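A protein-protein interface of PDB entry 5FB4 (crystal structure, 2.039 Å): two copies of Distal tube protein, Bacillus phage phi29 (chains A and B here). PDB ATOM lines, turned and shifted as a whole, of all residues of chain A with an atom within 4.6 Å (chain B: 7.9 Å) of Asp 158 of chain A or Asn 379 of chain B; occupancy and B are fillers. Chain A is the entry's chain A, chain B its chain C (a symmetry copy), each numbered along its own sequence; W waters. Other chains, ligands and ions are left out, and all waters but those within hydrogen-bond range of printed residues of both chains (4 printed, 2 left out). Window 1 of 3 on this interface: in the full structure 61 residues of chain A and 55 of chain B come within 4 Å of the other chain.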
ATOM      1  N   GLU A 156     -20.803  -9.413   4.935  1.00  0.00           N
ATOM      2  CA  GLU A 156     -22.258  -9.172   4.941  1.00  0.00           C
ATOM      3  C   GLU A 156     -22.945  -9.648   3.660  1.00  0.00           C
ATOM      4  O   GLU A 156     -22.312  -9.720   2.609  1.00  0.00           O
ATOM      5  CB  GLU A 156     -22.547  -7.676   5.124  1.00  0.00           C
ATOM      6  CG  GLU A 156     -22.008  -7.048   6.388  1.00  0.00           C
ATOM      7  CD  GLU A 156     -22.740  -7.501   7.641  1.00  0.00           C
ATOM      8  OE1 GLU A 156     -22.132  -7.445   8.731  1.00  0.00           O
ATOM      9  OE2 GLU A 156     -23.927  -7.876   7.542  1.00  0.00           O
ATOM     10  N   TYR A 157     -24.246  -9.937   3.743  1.00  0.00           N
ATOM     11  CA  TYR A 157     -25.042 -10.232   2.558  1.00  0.00           C
ATOM     12  C   TYR A 157     -25.892  -9.040   2.163  1.00  0.00           C
ATOM     13  O   TYR A 157     -26.324  -8.286   3.029  1.00  0.00           O
ATOM     14  CB  TYR A 157     -25.971 -11.408   2.798  1.00  0.00           C
ATOM     15  CG  TYR A 157     -25.313 -12.752   2.993  1.00  0.00           C
ATOM     16  CD1 TYR A 157     -24.674 -13.401   1.944  1.00  0.00           C
ATOM     17  CD2 TYR A 157     -25.377 -13.396   4.226  1.00  0.00           C
ATOM     18  CE1 TYR A 157     -24.088 -14.650   2.129  1.00  0.00           C
ATOM     19  CE2 TYR A 157     -24.797 -14.641   4.422  1.00  0.00           C
ATOM     20  CZ  TYR A 157     -24.156 -15.265   3.377  1.00  0.00           C
ATOM     21  OH  TYR A 157     -23.586 -16.507   3.577  1.00  0.00           O
ATOM     22  N   ASP A 158     -26.155  -8.900   0.864  1.00  0.00           N
ATOM     23  CA  ASP A 158     -27.248  -8.071   0.367  1.00  0.00           C
ATOM     24  C   ASP A 158     -28.553  -8.868   0.488  1.00  0.00           C
ATOM     25  O   ASP A 158     -28.592 -10.046   0.141  1.00  0.00           O
ATOM     26  CB  ASP A 158     -27.045  -7.677  -1.105  1.00  0.00           C
ATOM     27  CG  ASP A 158     -26.112  -6.490  -1.298  1.00  0.00           C
ATOM     28  OD1 ASP A 158     -25.957  -5.660  -0.379  1.00  0.00           O
ATOM     29  OD2 ASP A 158     -25.554  -6.366  -2.415  1.00  0.00           O
ATOM     30  N   ILE A 159     -29.612  -8.221   0.964  1.00  0.00           N
ATOM     31  CA  ILE A 159     -30.954  -8.782   0.886  1.00  0.00           C
ATOM     32  C   ILE A 159     -31.489  -8.483  -0.519  1.00  0.00           C
ATOM     33  O   ILE A 159     -31.602  -7.325  -0.915  1.00  0.00           O
ATOM     34  CB  ILE A 159     -31.879  -8.186   1.956  1.00  0.00           C
ATOM     35  CG1 ILE A 159     -31.353  -8.527   3.349  1.00  0.00           C
ATOM     36  CG2 ILE A 159     -33.300  -8.696   1.780  1.00  0.00           C
ATOM     37  CD1 ILE A 159     -31.737  -7.495   4.412  1.00  0.00           C
ATOM     38  N   VAL A 160     -31.772  -9.523  -1.290  1.00  0.00           N
ATOM     39  CA  VAL A 160     -32.137  -9.306  -2.688  1.00  0.00           C
ATOM     40  C   VAL A 160     -33.609  -9.640  -2.982  1.00  0.00           C
ATOM     41  O   VAL A 160     -34.173  -9.167  -3.967  1.00  0.00           O
ATOM     42  CB  VAL A 160     -31.192 -10.128  -3.620  1.00  0.00           C
ATOM     43  CG1 VAL A 160     -31.413 -11.638  -3.427  1.00  0.00           C
ATOM     44  CG2 VAL A 160     -31.370  -9.714  -5.059  1.00  0.00           C
ATOM     45  N   LYS A 515     -34.076 -13.796   0.689  1.00  0.00           N
ATOM     46  CA  LYS A 515     -32.933 -14.312  -0.077  1.00  0.00           C
ATOM     47  C   LYS A 515     -31.763 -13.341  -0.036  1.00  0.00           C
ATOM     48  O   LYS A 515     -31.932 -12.133  -0.174  1.00  0.00           O
ATOM     49  CB  LYS A 515     -33.359 -14.622  -1.507  1.00  0.00           C
ATOM     50  CG  LYS A 515     -34.429 -15.719  -1.495  1.00  0.00           C
ATOM     51  CD  LYS A 515     -34.912 -16.151  -2.864  1.00  0.00           C
ATOM     52  CE  LYS A 515     -36.081 -17.148  -2.675  1.00  0.00           C
ATOM     53  NZ  LYS A 515     -36.413 -17.873  -3.933  1.00  0.00           N
ATOM     54  N   LYS A 516     -30.578 -13.895   0.208  1.00  0.00           N
ATOM     55  CA  LYS A 516     -29.385 -13.109   0.493  1.00  0.00           C
ATOM     56  C   LYS A 516     -28.231 -13.570  -0.376  1.00  0.00           C
ATOM     57  O   LYS A 516     -28.106 -14.769  -0.628  1.00  0.00           O
ATOM     58  CB  LYS A 516     -28.984 -13.232   1.973  1.00  0.00           C
ATOM     59  CG  LYS A 516     -30.056 -12.775   2.961  1.00  0.00           C
ATOM     60  CD  LYS A 516     -29.569 -12.980   4.400  1.00  0.00           C
ATOM     61  CE  LYS A 516     -30.586 -12.451   5.401  1.00  0.00           C
ATOM     62  NZ  LYS A 516     -30.116 -12.625   6.801  1.00  0.00           N
ATOM     63  N   GLN A 517     -27.383 -12.628  -0.796  1.00  0.00           N
ATOM     64  CA  GLN A 517     -26.228 -12.953  -1.626  1.00  0.00           C
ATOM     65  C   GLN A 517     -25.041 -12.042  -1.320  1.00  0.00           C
ATOM     66  O   GLN A 517     -25.219 -10.931  -0.805  1.00  0.00           O
ATOM     67  CB  GLN A 517     -26.602 -12.850  -3.108  1.00  0.00           C
ATOM     68  CG  GLN A 517     -27.092 -11.472  -3.515  1.00  0.00           C
ATOM     69  CD  GLN A 517     -27.618 -11.462  -4.948  1.00  0.00           C
ATOM     70  OE1 GLN A 517     -28.144 -12.472  -5.439  1.00  0.00           O
ATOM     71  NE2 GLN A 517     -27.476 -10.325  -5.624  1.00  0.00           N
ATOM     72  N   LEU A 518     -23.839 -12.504  -1.657  1.00  0.00           N
ATOM     73  CA  LEU A 518     -22.616 -11.752  -1.338  1.00  0.00           C
ATOM     74  C   LEU A 518     -22.618 -10.401  -2.053  1.00  0.00           C
ATOM     75  O   LEU A 518     -23.324 -10.221  -3.056  1.00  0.00           O
ATOM     76  CB  LEU A 518     -21.360 -12.574  -1.704  1.00  0.00           C
ATOM     77  CG  LEU A 518     -20.952 -12.693  -3.176  1.00  0.00           C
ATOM     78  CD1 LEU A 518     -19.690 -13.568  -3.320  1.00  0.00           C
ATOM     79  CD2 LEU A 518     -22.095 -13.228  -4.059  1.00  0.00           C
ATOM     80  N   LYS A 519     -21.857  -9.452  -1.521  1.00  0.00           N
ATOM     81  CA  LYS A 519     -21.765  -8.109  -2.108  1.00  0.00           C
ATOM     82  C   LYS A 519     -21.080  -8.112  -3.475  1.00  0.00           C
ATOM     83  O   LYS A 519     -20.313  -9.018  -3.775  1.00  0.00           O
ATOM     84  CB  LYS A 519     -21.001  -7.182  -1.173  1.00  0.00           C
ATOM     85  CG  LYS A 519     -21.549  -7.088   0.257  1.00  0.00           C
ATOM     86  CD  LYS A 519     -22.835  -6.286   0.297  1.00  0.00           C
ATOM     87  CE  LYS A 519     -23.296  -6.025   1.753  1.00  0.00           C
ATOM     88  NZ  LYS A 519     -24.498  -5.169   1.728  1.00  0.00           N
ATOM     89  N   ASN B 346     -24.049  -2.145  15.611  1.00  0.00           N
ATOM     90  CA  ASN B 346     -23.023  -1.530  14.779  1.00  0.00           C
ATOM     91  C   ASN B 346     -23.412  -1.628  13.315  1.00  0.00           C
ATOM     92  O   ASN B 346     -23.824  -2.685  12.856  1.00  0.00           O
ATOM     93  CB  ASN B 346     -21.668  -2.206  15.005  1.00  0.00           C
ATOM     94  CG  ASN B 346     -20.971  -1.709  16.250  1.00  0.00           C
ATOM     95  OD1 ASN B 346     -21.372  -0.709  16.837  1.00  0.00           O
ATOM     96  ND2 ASN B 346     -19.921  -2.405  16.661  1.00  0.00           N
ATOM     97  N   LEU B 347     -23.326  -0.517  12.594  1.00  0.00           N
ATOM     98  CA  LEU B 347     -23.581  -0.531  11.157  1.00  0.00           C
ATOM     99  C   LEU B 347     -22.302  -0.236  10.391  1.00  0.00           C
ATOM    100  O   LEU B 347     -21.584   0.720  10.715  1.00  0.00           O
ATOM    101  CB  LEU B 347     -24.650   0.489  10.760  1.00  0.00           C
ATOM    102  CG  LEU B 347     -26.026   0.339  11.423  1.00  0.00           C
ATOM    103  CD1 LEU B 347     -26.974   1.347  10.843  1.00  0.00           C
ATOM    104  CD2 LEU B 347     -26.562  -1.073  11.237  1.00  0.00           C
ATOM    105  N   LYS B 348     -22.018  -1.063   9.389  1.00  0.00           N
ATOM    106  CA  LYS B 348     -20.954  -0.759   8.419  1.00  0.00           C
ATOM    107  C   LYS B 348     -21.485   0.258   7.436  1.00  0.00           C
ATOM    108  O   LYS B 348     -22.293  -0.065   6.567  1.00  0.00           O
ATOM    109  CB  LYS B 348     -20.500  -2.036   7.717  1.00  0.00           C
ATOM    110  CG  LYS B 348     -20.057  -3.055   8.748  1.00  0.00           C
ATOM    111  CD  LYS B 348     -19.804  -4.436   8.186  1.00  0.00           C
ATOM    112  CE  LYS B 348     -19.524  -5.369   9.378  1.00  0.00           C
ATOM    113  NZ  LYS B 348     -19.439  -6.779   8.985  1.00  0.00           N
ATOM    114  N   THR B 349     -21.030   1.497   7.602  1.00  0.00           N
ATOM    115  CA  THR B 349     -21.628   2.648   6.938  1.00  0.00           C
ATOM    116  C   THR B 349     -21.681   2.468   5.435  1.00  0.00           C
ATOM    117  O   THR B 349     -22.651   2.869   4.794  1.00  0.00           O
ATOM    118  CB  THR B 349     -20.847   3.932   7.286  1.00  0.00           C
ATOM    119  OG1 THR B 349     -20.636   3.969   8.699  1.00  0.00           O
ATOM    120  CG2 THR B 349     -21.602   5.200   6.837  1.00  0.00           C
ATOM    121  N   GLU B 350     -20.634   1.865   4.875  1.00  0.00           N
ATOM    122  CA  GLU B 350     -20.573   1.635   3.428  1.00  0.00           C
ATOM    123  C   GLU B 350     -21.725   0.753   2.930  1.00  0.00           C
ATOM    124  O   GLU B 350     -22.046   0.769   1.747  1.00  0.00           O
ATOM    125  CB  GLU B 350     -19.229   1.003   3.031  1.00  0.00           C
ATOM    126  CG  GLU B 350     -18.943  -0.327   3.716  1.00  0.00           C
ATOM    127  CD  GLU B 350     -18.180  -0.174   5.045  1.00  0.00           C
ATOM    128  OE1 GLU B 350     -17.398  -1.088   5.381  1.00  0.00           O
ATOM    129  OE2 GLU B 350     -18.368   0.842   5.753  1.00  0.00           O
ATOM    130  N   TYR B 351     -22.351  -0.006   3.829  1.00  0.00           N
ATOM    131  CA  TYR B 351     -23.400  -0.951   3.417  1.00  0.00           C
ATOM    132  C   TYR B 351     -24.813  -0.417   3.677  1.00  0.00           C
ATOM    133  O   TYR B 351     -25.809  -1.106   3.435  1.00  0.00           O
ATOM    134  CB  TYR B 351     -23.203  -2.295   4.113  1.00  0.00           C
ATOM    135  CG  TYR B 351     -21.980  -3.070   3.633  1.00  0.00           C
ATOM    136  CD1 TYR B 351     -21.490  -2.907   2.342  1.00  0.00           C
ATOM    137  CD2 TYR B 351     -21.327  -3.969   4.475  1.00  0.00           C
ATOM    138  CE1 TYR B 351     -20.366  -3.630   1.892  1.00  0.00           C
ATOM    139  CE2 TYR B 351     -20.208  -4.694   4.042  1.00  0.00           C
ATOM    140  CZ  TYR B 351     -19.737  -4.522   2.748  1.00  0.00           C
ATOM    141  OH  TYR B 351     -18.637  -5.256   2.310  1.00  0.00           O
ATOM    142  N   ILE B 352     -24.899   0.830   4.132  1.00  0.00           N
ATOM    143  CA  ILE B 352     -26.171   1.552   4.121  1.00  0.00           C
ATOM    144  C   ILE B 352     -26.457   1.978   2.683  1.00  0.00           C
ATOM    145  O   ILE B 352     -25.759   2.841   2.143  1.00  0.00           O
ATOM    146  CB  ILE B 352     -26.137   2.782   5.034  1.00  0.00           C
ATOM    147  CG1 ILE B 352     -25.754   2.375   6.463  1.00  0.00           C
ATOM    148  CG2 ILE B 352     -27.471   3.537   4.974  1.00  0.00           C
ATOM    149  CD1 ILE B 352     -25.488   3.585   7.388  1.00  0.00           C
ATOM    150  N   ASN B 353     -27.460   1.369   2.055  1.00  0.00           N
ATOM    151  CA  ASN B 353     -27.686   1.595   0.623  1.00  0.00           C
ATOM    152  C   ASN B 353     -28.492   2.869   0.364  1.00  0.00           C
ATOM    153  O   ASN B 353     -29.644   2.824  -0.050  1.00  0.00           O
ATOM    154  CB  ASN B 353     -28.390   0.384  -0.016  1.00  0.00           C
ATOM    155  CG  ASN B 353     -28.384   0.446  -1.548  1.00  0.00           C
ATOM    156  OD1 ASN B 353     -29.429   0.474  -2.195  1.00  0.00           O
ATOM    157  ND2 ASN B 353     -27.204   0.513  -2.117  1.00  0.00           N
ATOM    158  N   VAL B 375     -32.986   0.655  10.290  1.00  0.00           N
ATOM    159  CA  VAL B 375     -32.321   1.320   9.167  1.00  0.00           C
ATOM    160  C   VAL B 375     -32.592   0.447   7.955  1.00  0.00           C
ATOM    161  O   VAL B 375     -31.817  -0.468   7.644  1.00  0.00           O
ATOM    162  CB  VAL B 375     -30.803   1.504   9.400  1.00  0.00           C
ATOM    163  CG1 VAL B 375     -30.133   2.168   8.186  1.00  0.00           C
ATOM    164  CG2 VAL B 375     -30.574   2.330  10.657  1.00  0.00           C
ATOM    165  N   GLN B 376     -33.713   0.705   7.281  1.00  0.00           N
ATOM    166  CA  GLN B 376     -34.174  -0.221   6.254  1.00  0.00           C
ATOM    167  C   GLN B 376     -33.210  -0.326   5.082  1.00  0.00           C
ATOM    168  O   GLN B 376     -33.232  -1.317   4.361  1.00  0.00           O
ATOM    169  CB  GLN B 376     -35.557   0.180   5.731  1.00  0.00           C
ATOM    170  CG  GLN B 376     -35.569   1.365   4.786  1.00  0.00           C
ATOM    171  CD  GLN B 376     -37.004   1.764   4.414  1.00  0.00           C
ATOM    172  OE1 GLN B 376     -37.921   1.549   5.192  1.00  0.00           O
ATOM    173  NE2 GLN B 376     -37.192   2.305   3.214  1.00  0.00           N
ATOM    174  N   ASP B 377     -32.370   0.688   4.884  1.00  0.00           N
ATOM    175  CA  ASP B 377     -31.432   0.657   3.760  1.00  0.00           C
ATOM    176  C   ASP B 377     -30.177  -0.195   4.042  1.00  0.00           C
ATOM    177  O   ASP B 377     -29.357  -0.422   3.138  1.00  0.00           O
ATOM    178  CB  ASP B 377     -31.015   2.083   3.390  1.00  0.00           C
ATOM    179  CG  ASP B 377     -32.194   2.924   2.904  1.00  0.00           C
ATOM    180  OD1 ASP B 377     -33.035   2.398   2.136  1.00  0.00           O
ATOM    181  OD2 ASP B 377     -32.285   4.103   3.309  1.00  0.00           O
ATOM    182  N   TYR B 378     -30.019  -0.667   5.278  1.00  0.00           N
ATOM    183  CA  TYR B 378     -28.811  -1.430   5.623  1.00  0.00           C
ATOM    184  C   TYR B 378     -28.818  -2.793   4.950  1.00  0.00           C
ATOM    185  O   TYR B 378     -29.750  -3.569   5.132  1.00  0.00           O
ATOM    186  CB  TYR B 378     -28.665  -1.609   7.137  1.00  0.00           C
ATOM    187  CG  TYR B 378     -27.292  -2.133   7.560  1.00  0.00           C
ATOM    188  CD1 TYR B 378     -26.130  -1.440   7.211  1.00  0.00           C
ATOM    189  CD2 TYR B 378     -27.160  -3.298   8.297  1.00  0.00           C
ATOM    190  CE1 TYR B 378     -24.872  -1.902   7.588  1.00  0.00           C
ATOM    191  CE2 TYR B 378     -25.901  -3.770   8.692  1.00  0.00           C
ATOM    192  CZ  TYR B 378     -24.761  -3.053   8.330  1.00  0.00           C
ATOM    193  OH  TYR B 378     -23.511  -3.494   8.699  1.00  0.00           O
ATOM    194  N   ASN B 379     -27.776  -3.065   4.163  1.00  0.00           N
ATOM    195  CA  ASN B 379     -27.643  -4.328   3.437  1.00  0.00           C
ATOM    196  C   ASN B 379     -28.766  -4.609   2.454  1.00  0.00           C
ATOM    197  O   ASN B 379     -29.025  -5.753   2.118  1.00  0.00           O
ATOM    198  CB  ASN B 379     -27.527  -5.505   4.407  1.00  0.00           C
ATOM    199  CG  ASN B 379     -26.146  -5.593   5.037  1.00  0.00           C
ATOM    200  OD1 ASN B 379     -25.150  -5.206   4.419  1.00  0.00           O
ATOM    201  ND2 ASN B 379     -26.079  -6.103   6.269  1.00  0.00           N
ATOM    202  N   ALA B 380     -29.422  -3.557   1.990  1.00  0.00           N
ATOM    203  CA  ALA B 380     -30.444  -3.704   0.968  1.00  0.00           C
ATOM    204  C   ALA B 380     -29.797  -3.749  -0.408  1.00  0.00           C
ATOM    205  O   ALA B 380     -28.964  -2.902  -0.739  1.00  0.00           O
ATOM    206  CB  ALA B 380     -31.444  -2.554   1.040  1.00  0.00           C
ATOM    207  N   ASP B 381     -30.162  -4.732  -1.220  1.00  0.00           N
ATOM    208  CA  ASP B 381     -29.748  -4.687  -2.631  1.00  0.00           C
ATOM    209  C   ASP B 381     -30.331  -3.414  -3.272  1.00  0.00           C
ATOM    210  O   ASP B 381     -31.447  -3.002  -2.940  1.00  0.00           O
ATOM    211  CB  ASP B 381     -30.218  -5.929  -3.378  1.00  0.00           C
ATOM    212  CG  ASP B 381     -29.758  -5.939  -4.840  1.00  0.00           C
ATOM    213  OD1 ASP B 381     -28.567  -6.214  -5.082  1.00  0.00           O
ATOM    214  OD2 ASP B 381     -30.579  -5.661  -5.733  1.00  0.00           O
ATOM    215  N   SER B 382     -29.587  -2.773  -4.173  1.00  0.00           N
ATOM    216  CA  SER B 382     -30.064  -1.510  -4.763  1.00  0.00           C
ATOM    217  C   SER B 382     -31.454  -1.631  -5.413  1.00  0.00           C
ATOM    218  O   SER B 382     -32.220  -0.666  -5.426  1.00  0.00           O
ATOM    219  CB  SER B 382     -29.043  -0.964  -5.774  1.00  0.00           C
ATOM    220  OG  SER B 382     -28.702  -1.948  -6.736  1.00  0.00           O
ATOM    221  N   LEU B 384     -33.892  -3.550  -4.333  1.00  0.00           N
ATOM    222  CA  LEU B 384     -34.927  -3.910  -3.363  1.00  0.00           C
ATOM    223  C   LEU B 384     -35.830  -2.713  -3.078  1.00  0.00           C
ATOM    224  O   LEU B 384     -35.338  -1.630  -2.767  1.00  0.00           O
ATOM    225  CB  LEU B 384     -34.293  -4.420  -2.054  1.00  0.00           C
ATOM    226  CG  LEU B 384     -35.182  -5.212  -1.098  1.00  0.00           C
ATOM    227  CD1 LEU B 384     -35.668  -6.535  -1.723  1.00  0.00           C
ATOM    228  CD2 LEU B 384     -34.413  -5.467   0.189  1.00  0.00           C
ATOM    229  N   ARG B 389     -37.678  -3.399   1.926  1.00  0.00           N
ATOM    230  CA  ARG B 389     -36.637  -2.968   2.861  1.00  0.00           C
ATOM    231  C   ARG B 389     -37.192  -2.802   4.276  1.00  0.00           C
ATOM    232  O   ARG B 389     -36.637  -3.330   5.239  1.00  0.00           O
ATOM    233  CB  ARG B 389     -35.996  -1.653   2.412  1.00  0.00           C
ATOM    234  CG  ARG B 389     -35.080  -1.775   1.178  1.00  0.00           C
ATOM    235  CD  ARG B 389     -34.630  -0.390   0.691  1.00  0.00           C
ATOM    236  NE  ARG B 389     -33.953  -0.493  -0.598  1.00  0.00           N
ATOM    237  CZ  ARG B 389     -32.826   0.131  -0.936  1.00  0.00           C
ATOM    238  NH1 ARG B 389     -32.320  -0.071  -2.150  1.00  0.00           N
ATOM    239  NH2 ARG B 389     -32.195   0.934  -0.078  1.00  0.00           N
ATOM    240  N   ALA B 392     -38.071  -6.275   5.801  1.00  0.00           N
ATOM    241  CA  ALA B 392     -36.935  -7.131   6.131  1.00  0.00           C
ATOM    242  C   ALA B 392     -36.103  -6.587   7.285  1.00  0.00           C
ATOM    243  O   ALA B 392     -35.316  -7.306   7.880  1.00  0.00           O
ATOM    244  CB  ALA B 392     -36.041  -7.318   4.906  1.00  0.00           C
ATOM    245  N   SER B 396     -33.112  -6.963  12.278  1.00  0.00           N
ATOM    246  CA  SER B 396     -31.889  -6.261  12.654  1.00  0.00           C
ATOM    247  C   SER B 396     -32.182  -4.842  13.166  1.00  0.00           C
ATOM    248  O   SER B 396     -31.450  -3.908  12.861  1.00  0.00           O
ATOM    249  CB  SER B 396     -30.912  -6.219  11.475  1.00  0.00           C
ATOM    250  OG  SER B 396     -31.522  -5.658  10.338  1.00  0.00           O
HETATM  251  O   HOH W   1     -26.628  -7.838  -4.368  1.00  0.00           O
HETATM  252  O   HOH W   2     -33.515  -6.962  -5.206  1.00  0.00           O
HETATM  253  O   HOH W   3     -19.240  -8.065   2.699  1.00  0.00           O
HETATM  254  O   HOH W   4     -26.323  -3.343  -1.403  1.00  0.00           O
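Among the printed residues, pairs that only touch across the chains: Glu 156 of chain A with Tyr 351 of chain B (3.7 Å), Tyr 157 of chain A with Asn 379 of chain B (3.3 Å), Asp 158 of chain A with Asn 379 of chain B (3.4 Å), Ile 159 of chain A with Leu 384 of chain B (3.5 Å), Val 160 of chain A with Asp 381 of chain B (3.9 Å), Val 160 of chain A with Leu 384 of chain B (3.8 Å) and Lys 519 of chain A with Tyr 351 of chain B (3.7 Å).
Of the printed residues of chain B, Tyr 157 of chain A touches Asn 379 (3.3 Å). Of chain B, only Asn 379 (3.4 Å) comes within 4 Å of Asp 158 of chain A. Printed residues of chain B within 4 Å of Val 160 of chain A: Asp 381 and Leu 384. Of the printed residues of chain A, Lys 348 of chain B touches Glu 156. Of the printed residues of chain A, Tyr 351 of chain B touches Glu 156 and Lys 519. Of chain A, only Glu 156 (3.1 Å), Tyr 157 (3.3 Å), Asp 158 (3.4 Å), Ile 159 (2.8 Å) and Lys 519 (2.8 Å) come within 4 Å of Asn 379 of chain B. Of the printed residues of chain A, Asp 381 of chain B touches Ile 159 (3.0 Å) and Val 160 (3.9 Å).
No position is printed for both chains.
The backbone NH (N) of Asp 158 of chain A sits at hydrogen-bond distance from the backbone carbonyl oxygen (O) of Gln 517 of chain A (2.8 Å). The side-chain amino group (NZ) of Lys 519 of chain A is in salt-bridge range of the side-chain carboxylate (OD1) of Asp 158 of chain A, at 2.6 Å. The backbone NH of Val 160 of chain A is in hydrogen-bond range of the backbone carbonyl oxygen of Lys 515 of chain A, at 2.8 Å. N of Lys 348 of chain B sits at hydrogen-bond distance from OH of Tyr 378 of chain B (2.9 Å). The backbone carbonyl oxygen (O) of Asp 381 of chain B sits at hydrogen-bond distance from the guanidinium group (NH1) of Arg 389 of chain B. The backbone carbonyl oxygen (O) of Leu 384 of chain B sits at hydrogen-bond distance from the guanidinium group (NE) of Arg 389 of chain B (2.8 Å).
OE1 of Glu 156 of chain A is in salt-bridge range of NZ of Lys 348 of chain B (2.8 Å). The side-chain carboxylate (OE2) of Glu 156 of chain A lies within hydrogen-bond range of the side-chain amide nitrogen (ND2) of Asn 379 of chain B (3.1 Å). The backbone NH of Ile 159 of chain A is in hydrogen-bond range of the backbone carbonyl oxygen of Asn 379 of chain B (2.8 Å). N of Asp 381 of chain B lies within hydrogen-bond range of O of Ile 159 of chain A, 3.0 Å away. NZ of Lys 519 of chain A sits at hydrogen-bond distance from OD1 of Asn 379 of chain B (2.8 Å).
Hydrophobic or aromatic side chains of chain A that line the printed part of chain B: Ile 159.
Water W4 lies within hydrogen-bond range of the side-chain carboxylate of Asp 158 of chain A (2.6 Å) and the backbone carbonyl oxygen of Ala 380 of chain B (2.8 Å). Water W2 bridges O of Val 160 of chain A and OD2 of Asp 381 of chain B. Water W1 lies within hydrogen-bond range of OD1 of Asp 381 of chain B (2.6 Å), OD2 of Asp 158 of chain A (2.7 Å) and NE2 of Gln 517 of chain A (2.9 Å). Water W3 bridges OH of Tyr 351 of chain B and N of Glu 156 of chain A.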
